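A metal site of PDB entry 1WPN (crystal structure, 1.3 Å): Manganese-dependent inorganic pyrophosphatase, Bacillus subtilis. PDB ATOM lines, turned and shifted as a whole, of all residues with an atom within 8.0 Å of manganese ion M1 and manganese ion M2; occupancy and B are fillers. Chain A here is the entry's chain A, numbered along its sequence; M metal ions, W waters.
Within 4 Å of manganese ion M1: His 9, Asp 13 and Asp 75.
Manganese ion M2 is bound by water W1 (2.0 Å), the side-chain carboxylate of Asp 15 (2.1 Å), the side-chain carboxylate of Asp 75 (2.2 Å), the side-chain carboxylate of Asp 149 (2.2 Å) and a ring nitrogen (NE2) of His 97 (2.2 Å).
Merely in contact with manganese ion M2: Thr 119 (3.99 Å) and His 98 (3.9996 Å).
Manganese ion M1 is bound by water W1 (2.1 Å), the side-chain carboxylate (OD1) of Asp 13 (2.1 Å), water W2 (2.2 Å), the side-chain carboxylate (OD1) of Asp 75 (2.2 Å), a ring nitrogen (NE2) of His 9 (2.2 Å) and the side-chain carboxylate (OD2) of Asp 13 (2.7 Å).
Manganese ion M1 has six donor atoms within binding distance.
N of Thr 16 sits close to OD2 of Asp 13 (3.0 Å).
The backbone NH of Thr 119 lies close to the side-chain carboxylate of Asp 15, at 2.9 Å.
The side-chain carboxylate (OD1) of Asp 15 is in hydrogen-bond range of the backbone NH (N) of Ala 120 (3.5 Å).
The side-chain hydroxyl of Ser 19 is in hydrogen-bond range of the side-chain carboxylate of Asp 15 (2.8 Å).
OD2 of Asp 75 sits close to OG1 of Thr 119, 3.2 Å away.
O of Asp 75 sits close to ND1 of His 98 (3.5 Å).
The side-chain carboxylate (OD2) of Asp 149 lies close to the side-chain sulfur (SG) of Cys 118, 3.8 Å away.
The backbone carbonyl oxygen (O) of Val 116 lies within hydrogen-bond range of a ring nitrogen (ND1) of His 97 (3.1 Å).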
ATOM      1  N   GLY A   8      22.775   1.912  32.797  1.00  0.00           N
ATOM      2  CA  GLY A   8      22.719   3.356  32.848  1.00  0.00           C
ATOM      3  C   GLY A   8      21.593   3.857  33.735  1.00  0.00           C
ATOM      4  O   GLY A   8      21.143   3.155  34.677  1.00  0.00           O
ATOM      5  N   HIS A   9      21.210   5.107  33.484  1.00  0.00           N
ATOM      6  CA  HIS A   9      20.327   5.790  34.433  1.00  0.00           C
ATOM      7  C   HIS A   9      18.831   5.450  34.299  1.00  0.00           C
ATOM      8  O   HIS A   9      18.373   4.896  33.290  1.00  0.00           O
ATOM      9  CB  HIS A   9      20.499   7.327  34.359  1.00  0.00           C
ATOM     10  CG  HIS A   9      20.459   7.908  32.958  1.00  0.00           C
ATOM     11  ND1 HIS A   9      19.294   8.004  32.223  1.00  0.00           N
ATOM     12  CD2 HIS A   9      21.447   8.407  32.168  1.00  0.00           C
ATOM     13  CE1 HIS A   9      19.567   8.542  31.035  1.00  0.00           C
ATOM     14  NE2 HIS A   9      20.869   8.806  30.969  1.00  0.00           N
ATOM     15  N   GLN A  10      18.075   5.841  35.321  1.00  0.00           N
ATOM     16  CA  GLN A  10      16.593   5.890  35.262  1.00  0.00           C
ATOM     17  C   GLN A  10      16.189   6.808  34.130  1.00  0.00           C
ATOM     18  O   GLN A  10      16.944   7.711  33.773  1.00  0.00           O
ATOM     19  CB  GLN A  10      16.022   6.489  36.559  1.00  0.00           C
ATOM     20  CG  GLN A  10      16.262   5.663  37.789  1.00  0.00           C
ATOM     21  CD  GLN A  10      15.573   6.234  39.029  1.00  0.00           C
ATOM     22  OE1 GLN A  10      14.360   6.568  38.985  1.00  0.00           O
ATOM     23  NE2 GLN A  10      16.292   6.284  40.135  1.00  0.00           N
ATOM     24  N   ASN A  11      14.974   6.628  33.609  1.00  0.00           N
ATOM     25  CA  ASN A  11      14.522   7.351  32.410  1.00  0.00           C
ATOM     26  C   ASN A  11      15.530   7.178  31.262  1.00  0.00           C
ATOM     27  O   ASN A  11      16.207   8.123  30.827  1.00  0.00           O
ATOM     28  CB  ASN A  11      14.231   8.832  32.706  1.00  0.00           C
ATOM     29  CG  ASN A  11      13.217   9.000  33.795  1.00  0.00           C
ATOM     30  OD1 ASN A  11      12.159   8.326  33.808  1.00  0.00           O
ATOM     31  ND2 ASN A  11      13.507   9.915  34.719  1.00  0.00           N
ATOM     32  N   PRO A  12      15.724   5.937  30.845  1.00  0.00           N
ATOM     33  CA  PRO A  12      16.854   5.657  29.938  1.00  0.00           C
ATOM     34  C   PRO A  12      16.812   6.406  28.625  1.00  0.00           C
ATOM     35  O   PRO A  12      15.688   6.566  28.042  1.00  0.00           O
ATOM     36  CB  PRO A  12      16.734   4.155  29.653  1.00  0.00           C
ATOM     37  CG  PRO A  12      15.515   3.684  30.342  1.00  0.00           C
ATOM     38  CD  PRO A  12      14.990   4.721  31.229  1.00  0.00           C
ATOM     39  N   ASP A  13      17.995   6.839  28.169  1.00  0.00           N
ATOM     40  CA  ASP A  13      18.130   7.350  26.828  1.00  0.00           C
ATOM     41  C   ASP A  13      18.956   6.334  26.023  1.00  0.00           C
ATOM     42  O   ASP A  13      19.415   5.303  26.552  1.00  0.00           O
ATOM     43  CB  ASP A  13      18.744   8.786  26.816  1.00  0.00           C
ATOM     44  CG  ASP A  13      20.000   8.886  27.648  1.00  0.00           C
ATOM     45  OD1 ASP A  13      20.342  10.030  28.160  1.00  0.00           O
ATOM     46  OD2 ASP A  13      20.769   7.910  27.801  1.00  0.00           O
ATOM     47  N   THR A  14      19.173   6.658  24.762  1.00  0.00           N
ATOM     48  CA  THR A  14      19.835   5.751  23.863  1.00  0.00           C
ATOM     49  C   THR A  14      21.266   5.455  24.326  1.00  0.00           C
ATOM     50  O   THR A  14      21.707   4.311  24.260  1.00  0.00           O
ATOM     51  CB  THR A  14      19.796   6.322  22.458  1.00  0.00           C
ATOM     52  OG1 THR A  14      18.453   6.395  22.033  1.00  0.00           O
ATOM     53  CG2 THR A  14      20.547   5.447  21.419  1.00  0.00           C
ATOM     54  N   ASP A  15      22.006   6.460  24.831  1.00  0.00           N
ATOM     55  CA  ASP A  15      23.358   6.196  25.306  1.00  0.00           C
ATOM     56  C   ASP A  15      23.298   5.212  26.486  1.00  0.00           C
ATOM     57  O   ASP A  15      24.130   4.311  26.588  1.00  0.00           O
ATOM     58  CB  ASP A  15      24.024   7.502  25.708  1.00  0.00           C
ATOM     59  CG  ASP A  15      25.494   7.360  26.000  1.00  0.00           C
ATOM     60  OD1 ASP A  15      26.156   6.444  25.439  1.00  0.00           O
ATOM     61  OD2 ASP A  15      26.051   8.194  26.752  1.00  0.00           O
ATOM     62  N   THR A  16      22.374   5.430  27.419  1.00  0.00           N
ATOM     63  CA  THR A  16      22.311   4.574  28.588  1.00  0.00           C
ATOM     64  C   THR A  16      21.966   3.133  28.249  1.00  0.00           C
ATOM     65  O   THR A  16      22.457   2.218  28.934  1.00  0.00           O
ATOM     66  CB  THR A  16      21.310   5.206  29.598  1.00  0.00           C
ATOM     67  OG1 THR A  16      22.025   5.807  30.673  1.00  0.00           O
ATOM     68  CG2 THR A  16      20.332   4.204  30.229  1.00  0.00           C
ATOM     69  N   ILE A  17      21.149   2.916  27.214  1.00  0.00           N
ATOM     70  CA  ILE A  17      20.852   1.533  26.835  1.00  0.00           C
ATOM     71  C   ILE A  17      22.004   0.931  26.020  1.00  0.00           C
ATOM     72  O   ILE A  17      22.481  -0.172  26.310  1.00  0.00           O
ATOM     73  CB  ILE A  17      19.514   1.528  26.021  1.00  0.00           C
ATOM     74  CG1 ILE A  17      18.323   1.982  26.903  1.00  0.00           C
ATOM     75  CG2 ILE A  17      19.304   0.188  25.365  1.00  0.00           C
ATOM     76  CD1 ILE A  17      18.001   1.054  28.077  1.00  0.00           C
ATOM     77  N   SER A  19      25.183   1.889  25.619  1.00  0.00           N
ATOM     78  CA  SER A  19      26.476   1.760  26.285  1.00  0.00           C
ATOM     79  C   SER A  19      26.456   0.608  27.290  1.00  0.00           C
ATOM     80  O   SER A  19      27.478  -0.013  27.497  1.00  0.00           O
ATOM     81  CB  SER A  19      26.869   3.048  26.970  1.00  0.00           C
ATOM     82  OG  SER A  19      27.294   3.980  25.989  1.00  0.00           O
ATOM     83  N   VAL A  74      27.092   2.908  33.696  1.00  0.00           N
ATOM     84  CA  VAL A  74      27.470   3.647  32.483  1.00  0.00           C
ATOM     85  C   VAL A  74      26.612   4.886  32.392  1.00  0.00           C
ATOM     86  O   VAL A  74      25.419   4.862  32.789  1.00  0.00           O
ATOM     87  CB  VAL A  74      27.335   2.787  31.202  1.00  0.00           C
ATOM     88  CG1 VAL A  74      28.382   1.658  31.263  1.00  0.00           C
ATOM     89  CG2 VAL A  74      25.939   2.219  31.005  1.00  0.00           C
ATOM     90  N   ASP A  75      27.187   5.969  31.839  1.00  0.00           N
ATOM     91  CA  ASP A  75      26.427   7.161  31.473  1.00  0.00           C
ATOM     92  C   ASP A  75      25.811   7.897  32.662  1.00  0.00           C
ATOM     93  O   ASP A  75      24.970   8.791  32.456  1.00  0.00           O
ATOM     94  CB  ASP A  75      25.313   6.794  30.438  1.00  0.00           C
ATOM     95  CG  ASP A  75      24.689   7.989  29.817  1.00  0.00           C
ATOM     96  OD1 ASP A  75      23.431   8.015  29.665  1.00  0.00           O
ATOM     97  OD2 ASP A  75      25.429   8.935  29.414  1.00  0.00           O
ATOM     98  N   HIS A  76      26.226   7.574  33.881  1.00  0.00           N
ATOM     99  CA  HIS A  76      25.730   8.320  35.048  1.00  0.00           C
ATOM    100  C   HIS A  76      26.620   7.937  36.228  1.00  0.00           C
ATOM    101  O   HIS A  76      27.270   6.902  36.229  1.00  0.00           O
ATOM    102  CB  HIS A  76      24.263   8.028  35.393  1.00  0.00           C
ATOM    103  CG  HIS A  76      24.033   6.692  36.028  1.00  0.00           C
ATOM    104  ND1 HIS A  76      24.224   5.484  35.381  1.00  0.00           N
ATOM    105  CD2 HIS A  76      23.594   6.370  37.266  1.00  0.00           C
ATOM    106  CE1 HIS A  76      23.939   4.478  36.199  1.00  0.00           C
ATOM    107  NE2 HIS A  76      23.529   4.974  37.346  1.00  0.00           N
ATOM    108  N   GLN A  81      20.031   9.297  40.000  1.00  0.00           N
ATOM    109  CA  GLN A  81      19.838   8.814  38.619  1.00  0.00           C
ATOM    110  C   GLN A  81      20.009   7.297  38.534  1.00  0.00           C
ATOM    111  O   GLN A  81      19.760   6.715  37.484  1.00  0.00           O
ATOM    112  CB  GLN A  81      20.831   9.473  37.664  1.00  0.00           C
ATOM    113  CG  GLN A  81      20.653  10.990  37.588  1.00  0.00           C
ATOM    114  CD  GLN A  81      21.702  11.634  36.696  1.00  0.00           C
ATOM    115  OE1 GLN A  81      22.495  10.936  36.036  1.00  0.00           O
ATOM    116  NE2 GLN A  81      21.743  12.988  36.677  1.00  0.00           N
ATOM    117  N   ILE A  95      31.669   4.297  33.910  1.00  0.00           N
ATOM    118  CA  ILE A  95      32.165   4.890  32.652  1.00  0.00           C
ATOM    119  C   ILE A  95      31.202   6.019  32.309  1.00  0.00           C
ATOM    120  O   ILE A  95      30.026   5.720  32.129  1.00  0.00           O
ATOM    121  CB  ILE A  95      32.209   3.864  31.468  1.00  0.00           C
ATOM    122  CG1 ILE A  95      32.766   2.494  31.909  1.00  0.00           C
ATOM    123  CG2 ILE A  95      33.003   4.468  30.313  1.00  0.00           C
ATOM    124  CD1 ILE A  95      34.217   2.489  32.353  1.00  0.00           C
ATOM    125  N   ASP A  96      31.648   7.254  32.219  1.00  0.00           N
ATOM    126  CA  ASP A  96      30.671   8.377  32.137  1.00  0.00           C
ATOM    127  C   ASP A  96      31.304   9.612  31.511  1.00  0.00           C
ATOM    128  O   ASP A  96      32.508   9.693  31.299  1.00  0.00           O
ATOM    129  CB  ASP A  96      30.194   8.697  33.586  1.00  0.00           C
ATOM    130  CG  ASP A  96      29.050   9.673  33.614  1.00  0.00           C
ATOM    131  OD1 ASP A  96      28.972  10.449  34.595  1.00  0.00           O
ATOM    132  OD2 ASP A  96      28.199   9.653  32.695  1.00  0.00           O
ATOM    133  N   HIS A  97      30.444  10.587  31.207  1.00  0.00           N
ATOM    134  CA  HIS A  97      30.880  11.821  30.569  1.00  0.00           C
ATOM    135  C   HIS A  97      30.231  13.047  31.206  1.00  0.00           C
ATOM    136  O   HIS A  97      30.130  14.078  30.585  1.00  0.00           O
ATOM    137  CB  HIS A  97      30.630  11.768  29.030  1.00  0.00           C
ATOM    138  CG  HIS A  97      29.179  11.704  28.636  1.00  0.00           C
ATOM    139  ND1 HIS A  97      28.514  12.788  28.076  1.00  0.00           N
ATOM    140  CD2 HIS A  97      28.261  10.692  28.661  1.00  0.00           C
ATOM    141  CE1 HIS A  97      27.273  12.424  27.742  1.00  0.00           C
ATOM    142  NE2 HIS A  97      27.090  11.162  28.097  1.00  0.00           N
ATOM    143  N   HIS A  98      29.816  12.933  32.480  1.00  0.00           N
ATOM    144  CA  HIS A  98      29.136  14.022  33.186  1.00  0.00           C
ATOM    145  C   HIS A  98      29.926  14.526  34.360  1.00  0.00           C
ATOM    146  O   HIS A  98      30.936  13.914  34.776  1.00  0.00           O
ATOM    147  CB  HIS A  98      27.749  13.527  33.664  1.00  0.00           C
ATOM    148  CG  HIS A  98      26.844  13.092  32.557  1.00  0.00           C
ATOM    149  ND1 HIS A  98      26.731  11.785  32.169  1.00  0.00           N
ATOM    150  CD2 HIS A  98      26.070  13.816  31.705  1.00  0.00           C
ATOM    151  CE1 HIS A  98      25.873  11.696  31.139  1.00  0.00           C
ATOM    152  NE2 HIS A  98      25.469  12.931  30.844  1.00  0.00           N
ATOM    153  N   VAL A 116      33.719  14.327  27.072  1.00  0.00           N
ATOM    154  CA  VAL A 116      33.210  14.159  25.719  1.00  0.00           C
ATOM    155  C   VAL A 116      31.682  14.137  25.730  1.00  0.00           C
ATOM    156  O   VAL A 116      31.041  14.182  26.818  1.00  0.00           O
ATOM    157  CB  VAL A 116      33.760  12.877  25.064  1.00  0.00           C
ATOM    158  CG1 VAL A 116      35.272  12.976  24.918  1.00  0.00           C
ATOM    159  CG2 VAL A 116      33.395  11.612  25.870  1.00  0.00           C
ATOM    160  N   GLY A 117      31.092  14.054  24.531  1.00  0.00           N
ATOM    161  CA  GLY A 117      29.652  14.196  24.473  1.00  0.00           C
ATOM    162  C   GLY A 117      28.846  12.924  24.615  1.00  0.00           C
ATOM    163  O   GLY A 117      27.627  13.021  24.644  1.00  0.00           O
ATOM    164  N   CYS A 118      29.490  11.766  24.775  1.00  0.00           N
ATOM    165  CA  CYS A 118      28.723  10.505  24.812  1.00  0.00           C
ATOM    166  C   CYS A 118      29.550   9.414  25.441  1.00  0.00           C
ATOM    167  O   CYS A 118      30.758   9.362  25.203  1.00  0.00           O
ATOM    168  CB  CYS A 118      28.389  10.095  23.347  1.00  0.00           C
ATOM    169  SG  CYS A 118      27.378   8.621  23.226  1.00  0.00           S
ATOM    170  N   THR A 119      28.923   8.527  26.222  1.00  0.00           N
ATOM    171  CA  THR A 119      29.686   7.416  26.834  1.00  0.00           C
ATOM    172  C   THR A 119      30.272   6.497  25.786  1.00  0.00           C
ATOM    173  O   THR A 119      31.391   5.959  25.954  1.00  0.00           O
ATOM    174  CB  THR A 119      28.771   6.588  27.739  1.00  0.00           C
ATOM    175  OG1 THR A 119      28.161   7.484  28.693  1.00  0.00           O
ATOM    176  CG2 THR A 119      29.595   5.540  28.530  1.00  0.00           C
ATOM    177  N   ALA A 120      29.563   6.343  24.664  1.00  0.00           N
ATOM    178  CA  ALA A 120      30.003   5.370  23.654  1.00  0.00           C
ATOM    179  C   ALA A 120      31.354   5.789  23.004  1.00  0.00           C
ATOM    180  O   ALA A 120      32.095   4.914  22.557  1.00  0.00           O
ATOM    181  CB  ALA A 120      28.933   5.202  22.607  1.00  0.00           C
ATOM    182  N   ALA A 145      24.112   5.828  20.008  1.00  0.00           N
ATOM    183  CA  ALA A 145      24.337   6.600  21.235  1.00  0.00           C
ATOM    184  C   ALA A 145      24.968   7.979  20.956  1.00  0.00           C
ATOM    185  O   ALA A 145      24.470   8.980  21.487  1.00  0.00           O
ATOM    186  CB  ALA A 145      25.264   5.815  22.148  1.00  0.00           C
ATOM    187  N   ILE A 146      25.978   8.033  20.098  1.00  0.00           N
ATOM    188  CA  ILE A 146      26.619   9.299  19.799  1.00  0.00           C
ATOM    189  C   ILE A 146      25.680  10.222  19.059  1.00  0.00           C
ATOM    190  O   ILE A 146      25.621  11.400  19.379  1.00  0.00           O
ATOM    191  CB  ILE A 146      27.874   9.049  18.970  1.00  0.00           C
ATOM    192  CG1 ILE A 146      28.921   8.266  19.786  1.00  0.00           C
ATOM    193  CG2 ILE A 146      28.525  10.402  18.494  1.00  0.00           C
ATOM    194  CD1 ILE A 146      30.069   7.672  19.001  1.00  0.00           C
ATOM    195  N   SER A 148      22.425  10.261  19.236  1.00  0.00           N
ATOM    196  CA  SER A 148      21.442  10.662  20.194  1.00  0.00           C
ATOM    197  C   SER A 148      21.934  11.759  21.150  1.00  0.00           C
ATOM    198  O   SER A 148      21.304  12.816  21.268  1.00  0.00           O
ATOM    199  CB  SER A 148      21.014   9.451  21.015  1.00  0.00           C
ATOM    200  OG  SER A 148      20.111   9.857  22.025  1.00  0.00           O
ATOM    201  N   ASP A 149      23.091  11.515  21.775  1.00  0.00           N
ATOM    202  CA  ASP A 149      23.596  12.505  22.725  1.00  0.00           C
ATOM    203  C   ASP A 149      24.047  13.785  22.065  1.00  0.00           C
ATOM    204  O   ASP A 149      23.913  14.868  22.657  1.00  0.00           O
ATOM    205  CB  ASP A 149      24.732  11.932  23.539  1.00  0.00           C
ATOM    206  CG  ASP A 149      24.300  11.221  24.775  1.00  0.00           C
ATOM    207  OD1 ASP A 149      23.116  11.167  25.144  1.00  0.00           O
ATOM    208  OD2 ASP A 149      25.181  10.676  25.486  1.00  0.00           O
ATOM    209  N   SER A 150      24.569  13.675  20.857  1.00  0.00           N
ATOM    210  CA  SER A 150      25.069  14.870  20.151  1.00  0.00           C
ATOM    211  C   SER A 150      23.982  15.574  19.351  1.00  0.00           C
ATOM    212  O   SER A 150      24.283  16.619  18.755  1.00  0.00           O
ATOM    213  CB  SER A 150      26.220  14.504  19.243  1.00  0.00           C
ATOM    214  OG  SER A 150      25.706  13.822  18.095  1.00  0.00           O
HETATM  215 MN    MN M   1      22.098   9.667  29.301  1.00  0.00          MN
HETATM  216 MN    MN M   2      25.304  10.025  27.550  1.00  0.00          MN
HETATM  217  O   HOH W   1      23.370  10.545  27.858  1.00  0.00           O
HETATM  218  O   HOH W   2      22.643  11.167  30.745  1.00  0.00           O
